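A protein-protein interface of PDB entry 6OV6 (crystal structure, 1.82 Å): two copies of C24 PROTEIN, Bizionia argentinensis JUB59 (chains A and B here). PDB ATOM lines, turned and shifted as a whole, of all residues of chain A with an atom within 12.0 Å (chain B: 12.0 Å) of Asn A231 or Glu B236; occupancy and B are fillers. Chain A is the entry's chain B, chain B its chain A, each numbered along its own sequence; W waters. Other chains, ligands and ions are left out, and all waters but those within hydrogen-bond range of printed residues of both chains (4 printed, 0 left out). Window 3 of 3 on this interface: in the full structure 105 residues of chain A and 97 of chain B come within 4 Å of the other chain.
Among the printed residues, merely in contact across the chains: Ser A208 with Ser B241 (3.8 Å), Thr A209 with Arg B239 (3.8 Å), Thr A209 with Ala B240 (3.3 Å), Phe A210 with Ser B241 (3.7 Å), Gly A211 with Arg B239 (3.5 Å), Ser A212 with Arg B239 (3.5 Å), Gly A213 with Tyr B234 (3.2 Å), Gly A213 with Leu B235 (3.2 Å), Gly A213 with Leu B238 (3.9 Å), Leu A214 with Tyr B234 (3.3 Å), Leu A214 with Leu B238 (3.6 Å), Gly A215 with Tyr B234 (3.5 Å), Ala A216 with Gln B229 (3.9 Å), Val A217 with Ala B240 (3.8 Å), Val A223 with Leu B238 (3.9 Å), Val A223 with Arg B239 (3.6 Å), Val A224 with Leu B238 (3.5 Å), Val A224 with Ala B240 (3.7 Å), Val A224 with Ser B241 (3.8 Å), Gly A225 with Ser B237 (3.6 Å), Ser A226 with Leu B238 (3.9 Å), Ser A226 with Arg B239 (3.5 Å), Gln A228 with Ser B237 (3.3 Å), Glu A230 with Tyr B234 (3.5 Å), Glu A230 with Leu B235 (3.3 Å), Asn A231 with Glu B236 (3.4 Å), Leu A235 with Ser B237 (3.8 Å) and Leu A238 with Leu B238 (3.9 Å).
Printed residues of chain A that touch a printed residue of chain B: Ser A208, Thr A209, Phe A210, Gly A211, Ser A212, Gly A213, Leu A214, Gly A215, Ala A216, Val A217, Val A223, Val A224, Gly A225, Ser A226, Gln A228, Glu A230, Asn A231, Leu A235 and Leu A238.
Printed residues of chain B that touch a printed residue of chain A: Gln B229, Tyr B234, Leu B235, Glu B236, Ser B237, Leu B238, Arg B239, Ala B240 and Ser B241.
Among the printed residues, 37 pairs touch across the chains.
Among the printed residues, no Asp or Glu carboxylate lies within 4 Å of a Lys or Arg side-chain nitrogen of the other chain.
The guanidinium group (NH2) of Arg B239 lies within salt-bridge range of the side-chain carboxylate (OE2) of Glu B236 (2.8 Å).
The side-chain hydroxyl of Ser A226 is in hydrogen-bond range of the backbone NH of Gln A228 (3.1 Å).
Water W1 lies within hydrogen-bond range of the backbone carbonyl oxygen (O) of Phe A210 (2.6 Å), the backbone carbonyl oxygen (O) of Ser A212 (2.7 Å) and the backbone NH (N) of Ala B240 (3.0 Å).
Water W2 lies within hydrogen-bond range of the backbone carbonyl oxygen (O) of Gln A228 (2.7 Å), the backbone carbonyl oxygen (O) of Ser B237 (2.8 Å), the backbone NH (N) of Gly A227 (3.2 Å) and the side-chain hydroxyl (OG) of Ser A226 (3.4 Å).
Water W3 lies within hydrogen-bond range of N of Gly A215, O of Glu B230 and O of Ser B232.
Water W4 lies within hydrogen-bond range of O of Gly A215 (2.8 Å) and N of Glu B230 (2.9 Å).
Glu A230 touches Tyr B234, but with the chains exchanged Tyr A234 does not touch Glu B230 (12.7 Å).
Glu A230 touches Leu B235, but with the chains exchanged Leu A235 does not touch Glu B230 (9.5 Å).
Glu A230 touches Glu B236, but with the chains exchanged Glu A236 does not touch Glu B230 (13.5 Å).
Leu B238 touches its own counterpart, Leu A238.
Positions printed for both chains: 229, 230, 232, 233, 234, 235, 236 and 238.
Of the 37 pairs that touch across the chains among the printed residues, 1 has its exchanged pair printed and touching as well.
The backbone NH (N) of Glu B236 is in hydrogen-bond range of the side-chain carboxylate (OE1) of Glu A230 (2.9 Å).
The backbone NH (N) of Leu B235 sits at hydrogen-bond distance from the backbone carbonyl oxygen (O) of Leu A214, at 2.8 Å.
The backbone carbonyl oxygen (O) of Ala B240 lies within hydrogen-bond range of the backbone NH (N) of Phe A210 (2.9 Å).
The backbone carbonyl oxygen (O) of Arg B239 lies within hydrogen-bond range of the backbone NH (N) of Val A224 (2.9 Å).
The side-chain carboxylate of Glu A230 is in hydrogen-bond range of the side-chain hydroxyl of Ser B237, at 2.7 Å.
The backbone carbonyl oxygen (O) of Glu B236 sits at hydrogen-bond distance from the side-chain hydroxyl (OG) of Ser A226, at 2.6 Å.
OE2 of Glu B236 sits at hydrogen-bond distance from NE2 of Gln A228.
The guanidinium group (NH1) of Arg B239 sits close to the backbone NH (N) of Gly A213 (3.5 Å).
The backbone carbonyl oxygen (O) of Ser B237 is in hydrogen-bond range of the backbone NH (N) of Ser A226 (3.0 Å).
Of chain B, only Glu B236 (3.4 Å) comes within 4 Å of Asn A231.
Glu B236 touches four residues of chain A.
Ser A212 touches just one residue of chain B: Arg B239 (3.5 Å).
Leu A214 touches just these residues of chain B: Tyr B234, Leu B235 and Leu B238.
Of chain B, only Glu B236 (2.6 Å), Ser B237 (3.0 Å), Leu B238 (3.9 Å) and Arg B239 (3.5 Å) come within 4 Å of Ser A226.
No residue of chain B comes within 4 Å of Gly A227.
Gln A228 touches two residues of chain B.
Glu A230 touches just these residues of chain B: Tyr B234 (3.5 Å), Leu B235 (3.3 Å), Glu B236 (2.9 Å) and Ser B237 (2.7 Å).
No residue of chain B comes within 4 Å of Ser A232.
Glu A233 touches none of the printed residues of chain B.
Ser B237 touches just these residues of chain A: Gly A225 (3.6 Å), Ser A226 (3.0 Å), Gln A228 (3.3 Å), Glu A230 (2.7 Å) and Leu A235 (3.8 Å).
Of the printed residues of chain A, Tyr B234 touches Gly A213, Leu A214, Gly A215 and Glu A230.
Of the printed residues of chain B, Leu A235 touches Ser B237 (3.8 Å).
Printed residues of chain B within 4 Å of Val A223: Leu B238 (3.9 Å) and Arg B239 (3.6 Å).
Tyr A234 touches none of the printed residues of chain B.
The nearest residue of chain B that does not touch Asn A231 is Tyr B234 (5.3 Å).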
ATOM      1  N   SER A 208     -37.894  -9.937  17.828  1.00  0.00           N
ATOM      2  CA  SER A 208     -37.198 -11.000  18.577  1.00  0.00           C
ATOM      3  C   SER A 208     -36.161 -11.683  17.665  1.00  0.00           C
ATOM      4  O   SER A 208     -35.840 -11.170  16.583  1.00  0.00           O
ATOM      5  CB  SER A 208     -38.190 -11.997  19.189  1.00  0.00           C
ATOM      6  OG  SER A 208     -37.549 -12.946  20.031  1.00  0.00           O
ATOM      7  N   THR A 209     -35.579 -12.792  18.122  1.00  0.00           N
ATOM      8  CA  THR A 209     -34.584 -13.513  17.323  1.00  0.00           C
ATOM      9  C   THR A 209     -34.850 -15.009  17.433  1.00  0.00           C
ATOM     10  O   THR A 209     -35.495 -15.467  18.383  1.00  0.00           O
ATOM     11  CB  THR A 209     -33.131 -13.198  17.781  1.00  0.00           C
ATOM     12  OG1 THR A 209     -32.964 -13.667  19.118  1.00  0.00           O
ATOM     13  CG2 THR A 209     -32.746 -11.700  17.670  1.00  0.00           C
ATOM     14  N   PHE A 210     -34.323 -15.769  16.475  1.00  0.00           N
ATOM     15  CA  PHE A 210     -34.417 -17.224  16.482  1.00  0.00           C
ATOM     16  C   PHE A 210     -33.052 -17.744  16.041  1.00  0.00           C
ATOM     17  O   PHE A 210     -32.449 -17.166  15.132  1.00  0.00           O
ATOM     18  CB  PHE A 210     -35.501 -17.734  15.505  1.00  0.00           C
ATOM     19  CG  PHE A 210     -35.422 -19.235  15.294  1.00  0.00           C
ATOM     20  CD1 PHE A 210     -35.800 -20.117  16.304  1.00  0.00           C
ATOM     21  CD2 PHE A 210     -34.871 -19.764  14.131  1.00  0.00           C
ATOM     22  CE1 PHE A 210     -35.661 -21.498  16.135  1.00  0.00           C
ATOM     23  CE2 PHE A 210     -34.735 -21.148  13.965  1.00  0.00           C
ATOM     24  CZ  PHE A 210     -35.138 -22.002  14.965  1.00  0.00           C
ATOM     25  N   GLY A 211     -32.597 -18.850  16.647  1.00  0.00           N
ATOM     26  CA  GLY A 211     -31.348 -19.497  16.238  1.00  0.00           C
ATOM     27  C   GLY A 211     -30.075 -18.723  16.523  1.00  0.00           C
ATOM     28  O   GLY A 211     -30.045 -17.867  17.406  1.00  0.00           O
ATOM     29  N   SER A 212     -29.010 -19.018  15.776  1.00  0.00           N
ATOM     30  CA  SER A 212     -27.703 -18.383  16.001  1.00  0.00           C
ATOM     31  C   SER A 212     -27.200 -17.595  14.794  1.00  0.00           C
ATOM     32  O   SER A 212     -27.970 -17.327  13.867  1.00  0.00           O
ATOM     33  CB  SER A 212     -26.681 -19.426  16.460  1.00  0.00           C
ATOM     34  OG  SER A 212     -26.677 -20.558  15.607  1.00  0.00           O
ATOM     35  N   GLY A 213     -25.921 -17.207  14.824  1.00  0.00           N
ATOM     36  CA  GLY A 213     -25.267 -16.478  13.748  1.00  0.00           C
ATOM     37  C   GLY A 213     -25.362 -17.197  12.410  1.00  0.00           C
ATOM     38  O   GLY A 213     -25.667 -18.393  12.353  1.00  0.00           O
ATOM     39  N   LEU A 214     -25.139 -16.461  11.329  1.00  0.00           N
ATOM     40  CA  LEU A 214     -25.261 -17.014   9.985  1.00  0.00           C
ATOM     41  C   LEU A 214     -23.947 -17.631   9.457  1.00  0.00           C
ATOM     42  O   LEU A 214     -22.992 -16.902   9.262  1.00  0.00           O
ATOM     43  CB  LEU A 214     -25.793 -15.951   9.023  1.00  0.00           C
ATOM     44  CG  LEU A 214     -27.305 -15.682   9.052  1.00  0.00           C
ATOM     45  CD1 LEU A 214     -27.812 -15.280  10.450  1.00  0.00           C
ATOM     46  CD2 LEU A 214     -27.635 -14.590   8.061  1.00  0.00           C
ATOM     47  N   GLY A 215     -23.911 -18.945   9.197  1.00  0.00           N
ATOM     48  CA  GLY A 215     -25.016 -19.879   9.363  1.00  0.00           C
ATOM     49  C   GLY A 215     -26.059 -19.686   8.277  1.00  0.00           C
ATOM     50  O   GLY A 215     -25.748 -19.192   7.191  1.00  0.00           O
ATOM     51  N   ALA A 216     -27.304 -20.051   8.556  1.00  0.00           N
ATOM     52  CA  ALA A 216     -28.367 -19.879   7.561  1.00  0.00           C
ATOM     53  C   ALA A 216     -29.636 -19.367   8.208  1.00  0.00           C
ATOM     54  O   ALA A 216     -29.835 -19.540   9.420  1.00  0.00           O
ATOM     55  CB  ALA A 216     -28.638 -21.185   6.828  1.00  0.00           C
ATOM     56  N   VAL A 217     -30.505 -18.755   7.390  1.00  0.00           N
ATOM     57  CA  VAL A 217     -31.835 -18.281   7.828  1.00  0.00           C
ATOM     58  C   VAL A 217     -32.823 -18.852   6.818  1.00  0.00           C
ATOM     59  O   VAL A 217     -32.525 -18.857   5.627  1.00  0.00           O
ATOM     60  CB  VAL A 217     -31.918 -16.720   7.917  1.00  0.00           C
ATOM     61  CG1 VAL A 217     -33.373 -16.228   8.096  1.00  0.00           C
ATOM     62  CG2 VAL A 217     -31.046 -16.187   9.041  1.00  0.00           C
ATOM     63  N   VAL A 223     -34.637 -11.004   8.320  1.00  0.00           N
ATOM     64  CA  VAL A 223     -33.379 -11.009   9.061  1.00  0.00           C
ATOM     65  C   VAL A 223     -33.372  -9.762   9.945  1.00  0.00           C
ATOM     66  O   VAL A 223     -33.770  -8.678   9.513  1.00  0.00           O
ATOM     67  CB  VAL A 223     -32.159 -11.065   8.097  1.00  0.00           C
ATOM     68  CG1 VAL A 223     -30.838 -10.815   8.846  1.00  0.00           C
ATOM     69  CG2 VAL A 223     -32.128 -12.398   7.351  1.00  0.00           C
ATOM     70  N   VAL A 224     -32.929  -9.927  11.187  1.00  0.00           N
ATOM     71  CA  VAL A 224     -32.851  -8.859  12.182  1.00  0.00           C
ATOM     72  C   VAL A 224     -31.439  -8.737  12.754  1.00  0.00           C
ATOM     73  O   VAL A 224     -30.610  -9.648  12.587  1.00  0.00           O
ATOM     74  CB  VAL A 224     -33.889  -9.092  13.328  1.00  0.00           C
ATOM     75  CG1 VAL A 224     -35.318  -9.041  12.801  1.00  0.00           C
ATOM     76  CG2 VAL A 224     -33.622 -10.405  14.079  1.00  0.00           C
ATOM     77  N   GLY A 225     -31.203  -7.640  13.471  1.00  0.00           N
ATOM     78  CA  GLY A 225     -29.962  -7.446  14.221  1.00  0.00           C
ATOM     79  C   GLY A 225     -29.898  -8.395  15.405  1.00  0.00           C
ATOM     80  O   GLY A 225     -30.932  -8.808  15.933  1.00  0.00           O
ATOM     81  N   SER A 226     -28.674  -8.829  15.781  1.00  0.00           N
ATOM     82  CA  SER A 226     -28.479  -9.706  16.946  1.00  0.00           C
ATOM     83  C   SER A 226     -28.144  -8.827  18.177  1.00  0.00           C
ATOM     84  O   SER A 226     -28.212  -9.301  19.310  1.00  0.00           O
ATOM     85  CB  SER A 226     -27.320 -10.671  16.707  1.00  0.00           C
ATOM     86  OG  SER A 226     -26.101  -9.957  16.690  1.00  0.00           O
ATOM     87  N   GLY A 227     -27.752  -7.583  17.917  1.00  0.00           N
ATOM     88  CA  GLY A 227     -27.343  -6.631  18.948  1.00  0.00           C
ATOM     89  C   GLY A 227     -25.837  -6.658  19.126  1.00  0.00           C
ATOM     90  O   GLY A 227     -25.245  -5.680  19.592  1.00  0.00           O
ATOM     91  N   GLN A 228     -25.196  -7.748  18.662  1.00  0.00           N
ATOM     92  CA  GLN A 228     -23.750  -7.955  18.764  1.00  0.00           C
ATOM     93  C   GLN A 228     -22.977  -7.426  17.573  1.00  0.00           C
ATOM     94  O   GLN A 228     -23.463  -7.489  16.439  1.00  0.00           O
ATOM     95  CB  GLN A 228     -23.434  -9.440  19.008  1.00  0.00           C
ATOM     96  CG  GLN A 228     -23.863  -9.912  20.393  1.00  0.00           C
ATOM     97  CD  GLN A 228     -23.343 -11.285  20.719  1.00  0.00           C
ATOM     98  OE1 GLN A 228     -22.127 -11.525  20.764  1.00  0.00           O
ATOM     99  NE2 GLN A 228     -24.255 -12.218  20.971  1.00  0.00           N
ATOM    100  N   GLN A 229     -21.749  -6.920  17.825  1.00  0.00           N
ATOM    101  CA  GLN A 229     -20.857  -6.398  16.789  1.00  0.00           C
ATOM    102  C   GLN A 229     -20.430  -7.541  15.882  1.00  0.00           C
ATOM    103  O   GLN A 229     -20.329  -8.684  16.348  1.00  0.00           O
ATOM    104  CB  GLN A 229     -19.595  -5.770  17.432  1.00  0.00           C
ATOM    105  CG  GLN A 229     -19.810  -4.374  18.023  1.00  0.00           C
ATOM    106  CD  GLN A 229     -19.883  -3.274  16.980  1.00  0.00           C
ATOM    107  OE1 GLN A 229     -20.727  -2.372  17.064  1.00  0.00           O
ATOM    108  NE2 GLN A 229     -18.990  -3.303  15.982  1.00  0.00           N
ATOM    109  N   GLU A 230     -20.172  -7.255  14.599  1.00  0.00           N
ATOM    110  CA  GLU A 230     -19.700  -8.315  13.715  1.00  0.00           C
ATOM    111  C   GLU A 230     -18.227  -8.609  14.046  1.00  0.00           C
ATOM    112  O   GLU A 230     -17.450  -7.675  14.245  1.00  0.00           O
ATOM    113  CB  GLU A 230     -19.871  -7.959  12.226  1.00  0.00           C
ATOM    114  CG  GLU A 230     -19.700  -9.152  11.299  1.00  0.00           C
ATOM    115  CD  GLU A 230     -20.455 -10.401  11.722  1.00  0.00           C
ATOM    116  OE1 GLU A 230     -19.829 -11.318  12.307  1.00  0.00           O
ATOM    117  OE2 GLU A 230     -21.691 -10.425  11.528  1.00  0.00           O
ATOM    118  N   ASN A 231     -17.869  -9.899  14.132  1.00  0.00           N
ATOM    119  CA  ASN A 231     -16.515 -10.338  14.466  1.00  0.00           C
ATOM    120  C   ASN A 231     -15.615 -10.287  13.239  1.00  0.00           C
ATOM    121  O   ASN A 231     -15.944 -10.878  12.206  1.00  0.00           O
ATOM    122  CB  ASN A 231     -16.532 -11.765  15.065  1.00  0.00           C
ATOM    123  CG  ASN A 231     -17.489 -11.991  16.221  1.00  0.00           C
ATOM    124  OD1 ASN A 231     -18.095 -13.057  16.340  1.00  0.00           O
ATOM    125  ND2 ASN A 231     -17.642 -11.014  17.109  1.00  0.00           N
ATOM    126  N   SER A 232     -14.482  -9.564  13.348  1.00  0.00           N
ATOM    127  CA  SER A 232     -13.432  -9.423  12.321  1.00  0.00           C
ATOM    128  C   SER A 232     -13.839  -8.873  10.936  1.00  0.00           C
ATOM    129  O   SER A 232     -12.957  -8.510  10.144  1.00  0.00           O
ATOM    130  CB  SER A 232     -12.645 -10.730  12.166  1.00  0.00           C
ATOM    131  OG  SER A 232     -13.426 -11.760  11.581  1.00  0.00           O
ATOM    132  N   GLU A 233     -15.147  -8.814  10.638  1.00  0.00           N
ATOM    133  CA  GLU A 233     -15.616  -8.367   9.333  1.00  0.00           C
ATOM    134  C   GLU A 233     -16.556  -7.163   9.359  1.00  0.00           C
ATOM    135  O   GLU A 233     -17.264  -6.960  10.348  1.00  0.00           O
ATOM    136  CB  GLU A 233     -16.232  -9.543   8.572  1.00  0.00           C
ATOM    137  CG  GLU A 233     -16.095  -9.411   7.067  1.00  0.00           C
ATOM    138  CD  GLU A 233     -14.696  -9.296   6.485  1.00  0.00           C
ATOM    139  OE1 GLU A 233     -13.913 -10.267   6.612  1.00  0.00           O
ATOM    140  OE2 GLU A 233     -14.411  -8.262   5.838  1.00  0.00           O
ATOM    141  N   TYR A 234     -16.551  -6.363   8.269  1.00  0.00           N
ATOM    142  CA  TYR A 234     -17.419  -5.199   8.124  1.00  0.00           C
ATOM    143  C   TYR A 234     -18.360  -5.336   6.919  1.00  0.00           C
ATOM    144  O   TYR A 234     -17.905  -5.387   5.780  1.00  0.00           O
ATOM    145  CB  TYR A 234     -16.600  -3.915   8.053  1.00  0.00           C
ATOM    146  CG  TYR A 234     -17.420  -2.670   8.280  1.00  0.00           C
ATOM    147  CD1 TYR A 234     -17.735  -2.243   9.568  1.00  0.00           C
ATOM    148  CD2 TYR A 234     -17.830  -1.880   7.210  1.00  0.00           C
ATOM    149  CE1 TYR A 234     -18.440  -1.062   9.786  1.00  0.00           C
ATOM    150  CE2 TYR A 234     -18.543  -0.700   7.414  1.00  0.00           C
ATOM    151  CZ  TYR A 234     -18.833  -0.288   8.706  1.00  0.00           C
ATOM    152  OH  TYR A 234     -19.536   0.875   8.915  1.00  0.00           O
ATOM    153  N   LEU A 235     -19.674  -5.387   7.191  1.00  0.00           N
ATOM    154  CA  LEU A 235     -20.734  -5.594   6.200  1.00  0.00           C
ATOM    155  C   LEU A 235     -21.322  -4.295   5.701  1.00  0.00           C
ATOM    156  O   LEU A 235     -22.188  -3.706   6.352  1.00  0.00           O
ATOM    157  CB  LEU A 235     -21.824  -6.571   6.721  1.00  0.00           C
ATOM    158  CG  LEU A 235     -21.336  -7.846   7.409  1.00  0.00           C
ATOM    159  CD1 LEU A 235     -22.488  -8.621   8.014  1.00  0.00           C
ATOM    160  CD2 LEU A 235     -20.482  -8.719   6.461  1.00  0.00           C
ATOM    161  N   GLU A 236     -20.790  -3.828   4.563  1.00  0.00           N
ATOM    162  CA  GLU A 236     -21.189  -2.581   3.918  1.00  0.00           C
ATOM    163  C   GLU A 236     -22.530  -2.684   3.168  1.00  0.00           C
ATOM    164  O   GLU A 236     -23.154  -1.665   2.914  1.00  0.00           O
ATOM    165  CB  GLU A 236     -20.077  -2.101   2.968  1.00  0.00           C
ATOM    166  CG  GLU A 236     -20.237  -0.687   2.412  1.00  0.00           C
ATOM    167  CD  GLU A 236     -20.723   0.441   3.317  1.00  0.00           C
ATOM    168  OE1 GLU A 236     -20.416   0.435   4.531  1.00  0.00           O
ATOM    169  OE2 GLU A 236     -21.396   1.353   2.790  1.00  0.00           O
ATOM    170  N   LEU A 238     -25.333  -3.938   4.203  1.00  0.00           N
ATOM    171  CA  LEU A 238     -26.473  -3.930   5.113  1.00  0.00           C
ATOM    172  C   LEU A 238     -26.533  -2.722   6.023  1.00  0.00           C
ATOM    173  O   LEU A 238     -25.504  -2.100   6.343  1.00  0.00           O
ATOM    174  CB  LEU A 238     -26.402  -5.194   6.001  1.00  0.00           C
ATOM    175  CG  LEU A 238     -26.303  -6.551   5.287  1.00  0.00           C
ATOM    176  CD1 LEU A 238     -25.982  -7.656   6.281  1.00  0.00           C
ATOM    177  CD2 LEU A 238     -27.627  -6.838   4.509  1.00  0.00           C
ATOM    178  N   GLN B 229     -26.437 -22.120   3.245  1.00  0.00           N
ATOM    179  CA  GLN B 229     -25.358 -22.020   4.211  1.00  0.00           C
ATOM    180  C   GLN B 229     -24.039 -22.199   3.472  1.00  0.00           C
ATOM    181  O   GLN B 229     -23.836 -23.221   2.808  1.00  0.00           O
ATOM    182  CB  GLN B 229     -25.513 -23.051   5.326  1.00  0.00           C
ATOM    183  CG  GLN B 229     -24.315 -23.055   6.268  1.00  0.00           C
ATOM    184  CD  GLN B 229     -24.510 -23.904   7.486  1.00  0.00           C
ATOM    185  OE1 GLN B 229     -25.457 -24.683   7.590  1.00  0.00           O
ATOM    186  NE2 GLN B 229     -23.586 -23.781   8.427  1.00  0.00           N
ATOM    187  N   GLU B 230     -23.184 -21.181   3.544  1.00  0.00           N
ATOM    188  CA  GLU B 230     -21.862 -21.153   2.925  1.00  0.00           C
ATOM    189  C   GLU B 230     -20.880 -21.731   3.950  1.00  0.00           C
ATOM    190  O   GLU B 230     -21.184 -21.722   5.146  1.00  0.00           O
ATOM    191  CB  GLU B 230     -21.482 -19.690   2.685  1.00  0.00           C
ATOM    192  CG  GLU B 230     -21.012 -19.308   1.296  1.00  0.00           C
ATOM    193  CD  GLU B 230     -20.589 -17.847   1.208  1.00  0.00           C
ATOM    194  OE1 GLU B 230     -21.260 -16.993   1.836  1.00  0.00           O
ATOM    195  OE2 GLU B 230     -19.578 -17.555   0.528  1.00  0.00           O
ATOM    196  N   SER B 232     -18.385 -20.539   5.593  1.00  0.00           N
ATOM    197  CA  SER B 232     -17.779 -19.242   5.869  1.00  0.00           C
ATOM    198  C   SER B 232     -17.745 -18.890   7.328  1.00  0.00           C
ATOM    199  O   SER B 232     -18.337 -19.580   8.170  1.00  0.00           O
ATOM    200  CB  SER B 232     -18.516 -18.151   5.089  1.00  0.00           C
ATOM    201  OG  SER B 232     -19.918 -18.218   5.317  1.00  0.00           O
ATOM    202  N   GLU B 233     -17.033 -17.786   7.629  1.00  0.00           N
ATOM    203  CA  GLU B 233     -16.939 -17.236   8.975  1.00  0.00           C
ATOM    204  C   GLU B 233     -18.362 -16.824   9.379  1.00  0.00           C
ATOM    205  O   GLU B 233     -19.047 -16.203   8.567  1.00  0.00           O
ATOM    206  CB  GLU B 233     -15.972 -16.027   8.991  1.00  0.00           C
ATOM    207  CG  GLU B 233     -14.518 -16.388   8.736  1.00  0.00           C
ATOM    208  CD  GLU B 233     -13.930 -17.346   9.757  1.00  0.00           C
ATOM    209  OE1 GLU B 233     -13.851 -18.559   9.452  1.00  0.00           O
ATOM    210  OE2 GLU B 233     -13.621 -16.898  10.885  1.00  0.00           O
ATOM    211  N   TYR B 234     -18.842 -17.282  10.555  1.00  0.00           N
ATOM    212  CA  TYR B 234     -20.190 -16.983  11.068  1.00  0.00           C
ATOM    213  C   TYR B 234     -20.454 -15.471  11.182  1.00  0.00           C
ATOM    214  O   TYR B 234     -19.550 -14.726  11.560  1.00  0.00           O
ATOM    215  CB  TYR B 234     -20.426 -17.659  12.433  1.00  0.00           C
ATOM    216  CG  TYR B 234     -21.359 -18.853  12.400  1.00  0.00           C
ATOM    217  CD1 TYR B 234     -22.339 -19.024  13.375  1.00  0.00           C
ATOM    218  CD2 TYR B 234     -21.219 -19.852  11.435  1.00  0.00           C
ATOM    219  CE1 TYR B 234     -23.173 -20.147  13.377  1.00  0.00           C
ATOM    220  CE2 TYR B 234     -22.055 -20.970  11.419  1.00  0.00           C
ATOM    221  CZ  TYR B 234     -23.028 -21.116  12.394  1.00  0.00           C
ATOM    222  OH  TYR B 234     -23.847 -22.223  12.371  1.00  0.00           O
ATOM    223  N   LEU B 235     -21.661 -15.025  10.774  1.00  0.00           N
ATOM    224  CA  LEU B 235     -22.082 -13.624  10.885  1.00  0.00           C
ATOM    225  C   LEU B 235     -22.810 -13.475  12.207  1.00  0.00           C
ATOM    226  O   LEU B 235     -23.960 -13.891  12.339  1.00  0.00           O
ATOM    227  CB  LEU B 235     -22.952 -13.174   9.685  1.00  0.00           C
ATOM    228  CG  LEU B 235     -22.338 -13.388   8.291  1.00  0.00           C
ATOM    229  CD1 LEU B 235     -23.346 -13.053   7.207  1.00  0.00           C
ATOM    230  CD2 LEU B 235     -21.060 -12.563   8.101  1.00  0.00           C
ATOM    231  N   GLU B 236     -22.097 -12.946  13.206  1.00  0.00           N
ATOM    232  CA  GLU B 236     -22.599 -12.777  14.568  1.00  0.00           C
ATOM    233  C   GLU B 236     -23.558 -11.593  14.729  1.00  0.00           C
ATOM    234  O   GLU B 236     -24.347 -11.592  15.670  1.00  0.00           O
ATOM    235  CB  GLU B 236     -21.408 -12.684  15.564  1.00  0.00           C
ATOM    236  CG  GLU B 236     -21.782 -12.680  17.047  1.00  0.00           C
ATOM    237  CD  GLU B 236     -22.783 -13.713  17.544  1.00  0.00           C
ATOM    238  OE1 GLU B 236     -22.843 -14.832  16.982  1.00  0.00           O
ATOM    239  OE2 GLU B 236     -23.504 -13.401  18.518  1.00  0.00           O
ATOM    240  N   SER B 237     -23.483 -10.598  13.819  1.00  0.00           N
ATOM    241  CA  SER B 237     -24.322  -9.399  13.862  1.00  0.00           C
ATOM    242  C   SER B 237     -25.782  -9.619  13.434  1.00  0.00           C
ATOM    243  O   SER B 237     -26.598  -8.704  13.582  1.00  0.00           O
ATOM    244  CB  SER B 237     -23.700  -8.284  13.031  1.00  0.00           C
ATOM    245  OG  SER B 237     -23.715  -8.600  11.650  1.00  0.00           O
ATOM    246  N   LEU B 238     -26.106 -10.825  12.926  1.00  0.00           N
ATOM    247  CA  LEU B 238     -27.430 -11.139  12.375  1.00  0.00           C
ATOM    248  C   LEU B 238     -28.090 -12.343  12.988  1.00  0.00           C
ATOM    249  O   LEU B 238     -27.422 -13.264  13.460  1.00  0.00           O
ATOM    250  CB  LEU B 238     -27.280 -11.385  10.847  1.00  0.00           C
ATOM    251  CG  LEU B 238     -26.645 -10.273  10.023  1.00  0.00           C
ATOM    252  CD1 LEU B 238     -26.327 -10.755   8.595  1.00  0.00           C
ATOM    253  CD2 LEU B 238     -27.553  -9.011  10.014  1.00  0.00           C
ATOM    254  N   ARG B 239     -29.430 -12.357  12.936  1.00  0.00           N
ATOM    255  CA  ARG B 239     -30.252 -13.476  13.354  1.00  0.00           C
ATOM    256  C   ARG B 239     -31.492 -13.511  12.497  1.00  0.00           C
ATOM    257  O   ARG B 239     -31.910 -12.486  11.948  1.00  0.00           O
ATOM    258  CB  ARG B 239     -30.718 -13.335  14.829  1.00  0.00           C
ATOM    259  CG  ARG B 239     -29.647 -13.424  15.926  1.00  0.00           C
ATOM    260  CD  ARG B 239     -28.996 -14.801  16.045  1.00  0.00           C
ATOM    261  NE  ARG B 239     -28.056 -14.868  17.163  1.00  0.00           N
ATOM    262  CZ  ARG B 239     -26.790 -14.471  17.118  1.00  0.00           C
ATOM    263  NH1 ARG B 239     -26.291 -13.954  16.009  1.00  0.00           N
ATOM    264  NH2 ARG B 239     -26.015 -14.581  18.191  1.00  0.00           N
ATOM    265  N   ALA B 240     -32.144 -14.675  12.470  1.00  0.00           N
ATOM    266  CA  ALA B 240     -33.463 -14.799  11.892  1.00  0.00           C
ATOM    267  C   ALA B 240     -34.371 -14.054  12.873  1.00  0.00           C
ATOM    268  O   ALA B 240     -34.119 -14.064  14.082  1.00  0.00           O
ATOM    269  CB  ALA B 240     -33.890 -16.269  11.874  1.00  0.00           C
ATOM    270  N   SER B 241     -35.438 -13.422  12.363  1.00  0.00           N
ATOM    271  CA  SER B 241     -36.475 -12.814  13.200  1.00  0.00           C
ATOM    272  C   SER B 241     -37.143 -13.972  13.990  1.00  0.00           C
ATOM    273  O   SER B 241     -37.163 -15.115  13.516  1.00  0.00           O
ATOM    274  CB  SER B 241     -37.523 -12.142  12.314  1.00  0.00           C
ATOM    275  OG  SER B 241     -37.907 -13.036  11.280  1.00  0.00           O
HETATM  276  O   HOH W   1     -30.614 -17.136  13.299  1.00  0.00           O
HETATM  277  O   HOH W   2     -25.868  -6.759  15.424  1.00  0.00           O
HETATM  278  O   HOH W   3     -21.734 -20.251   7.972  1.00  0.00           O
HETATM  279  O   HOH W   4     -23.451 -19.124   5.543  1.00  0.00           O
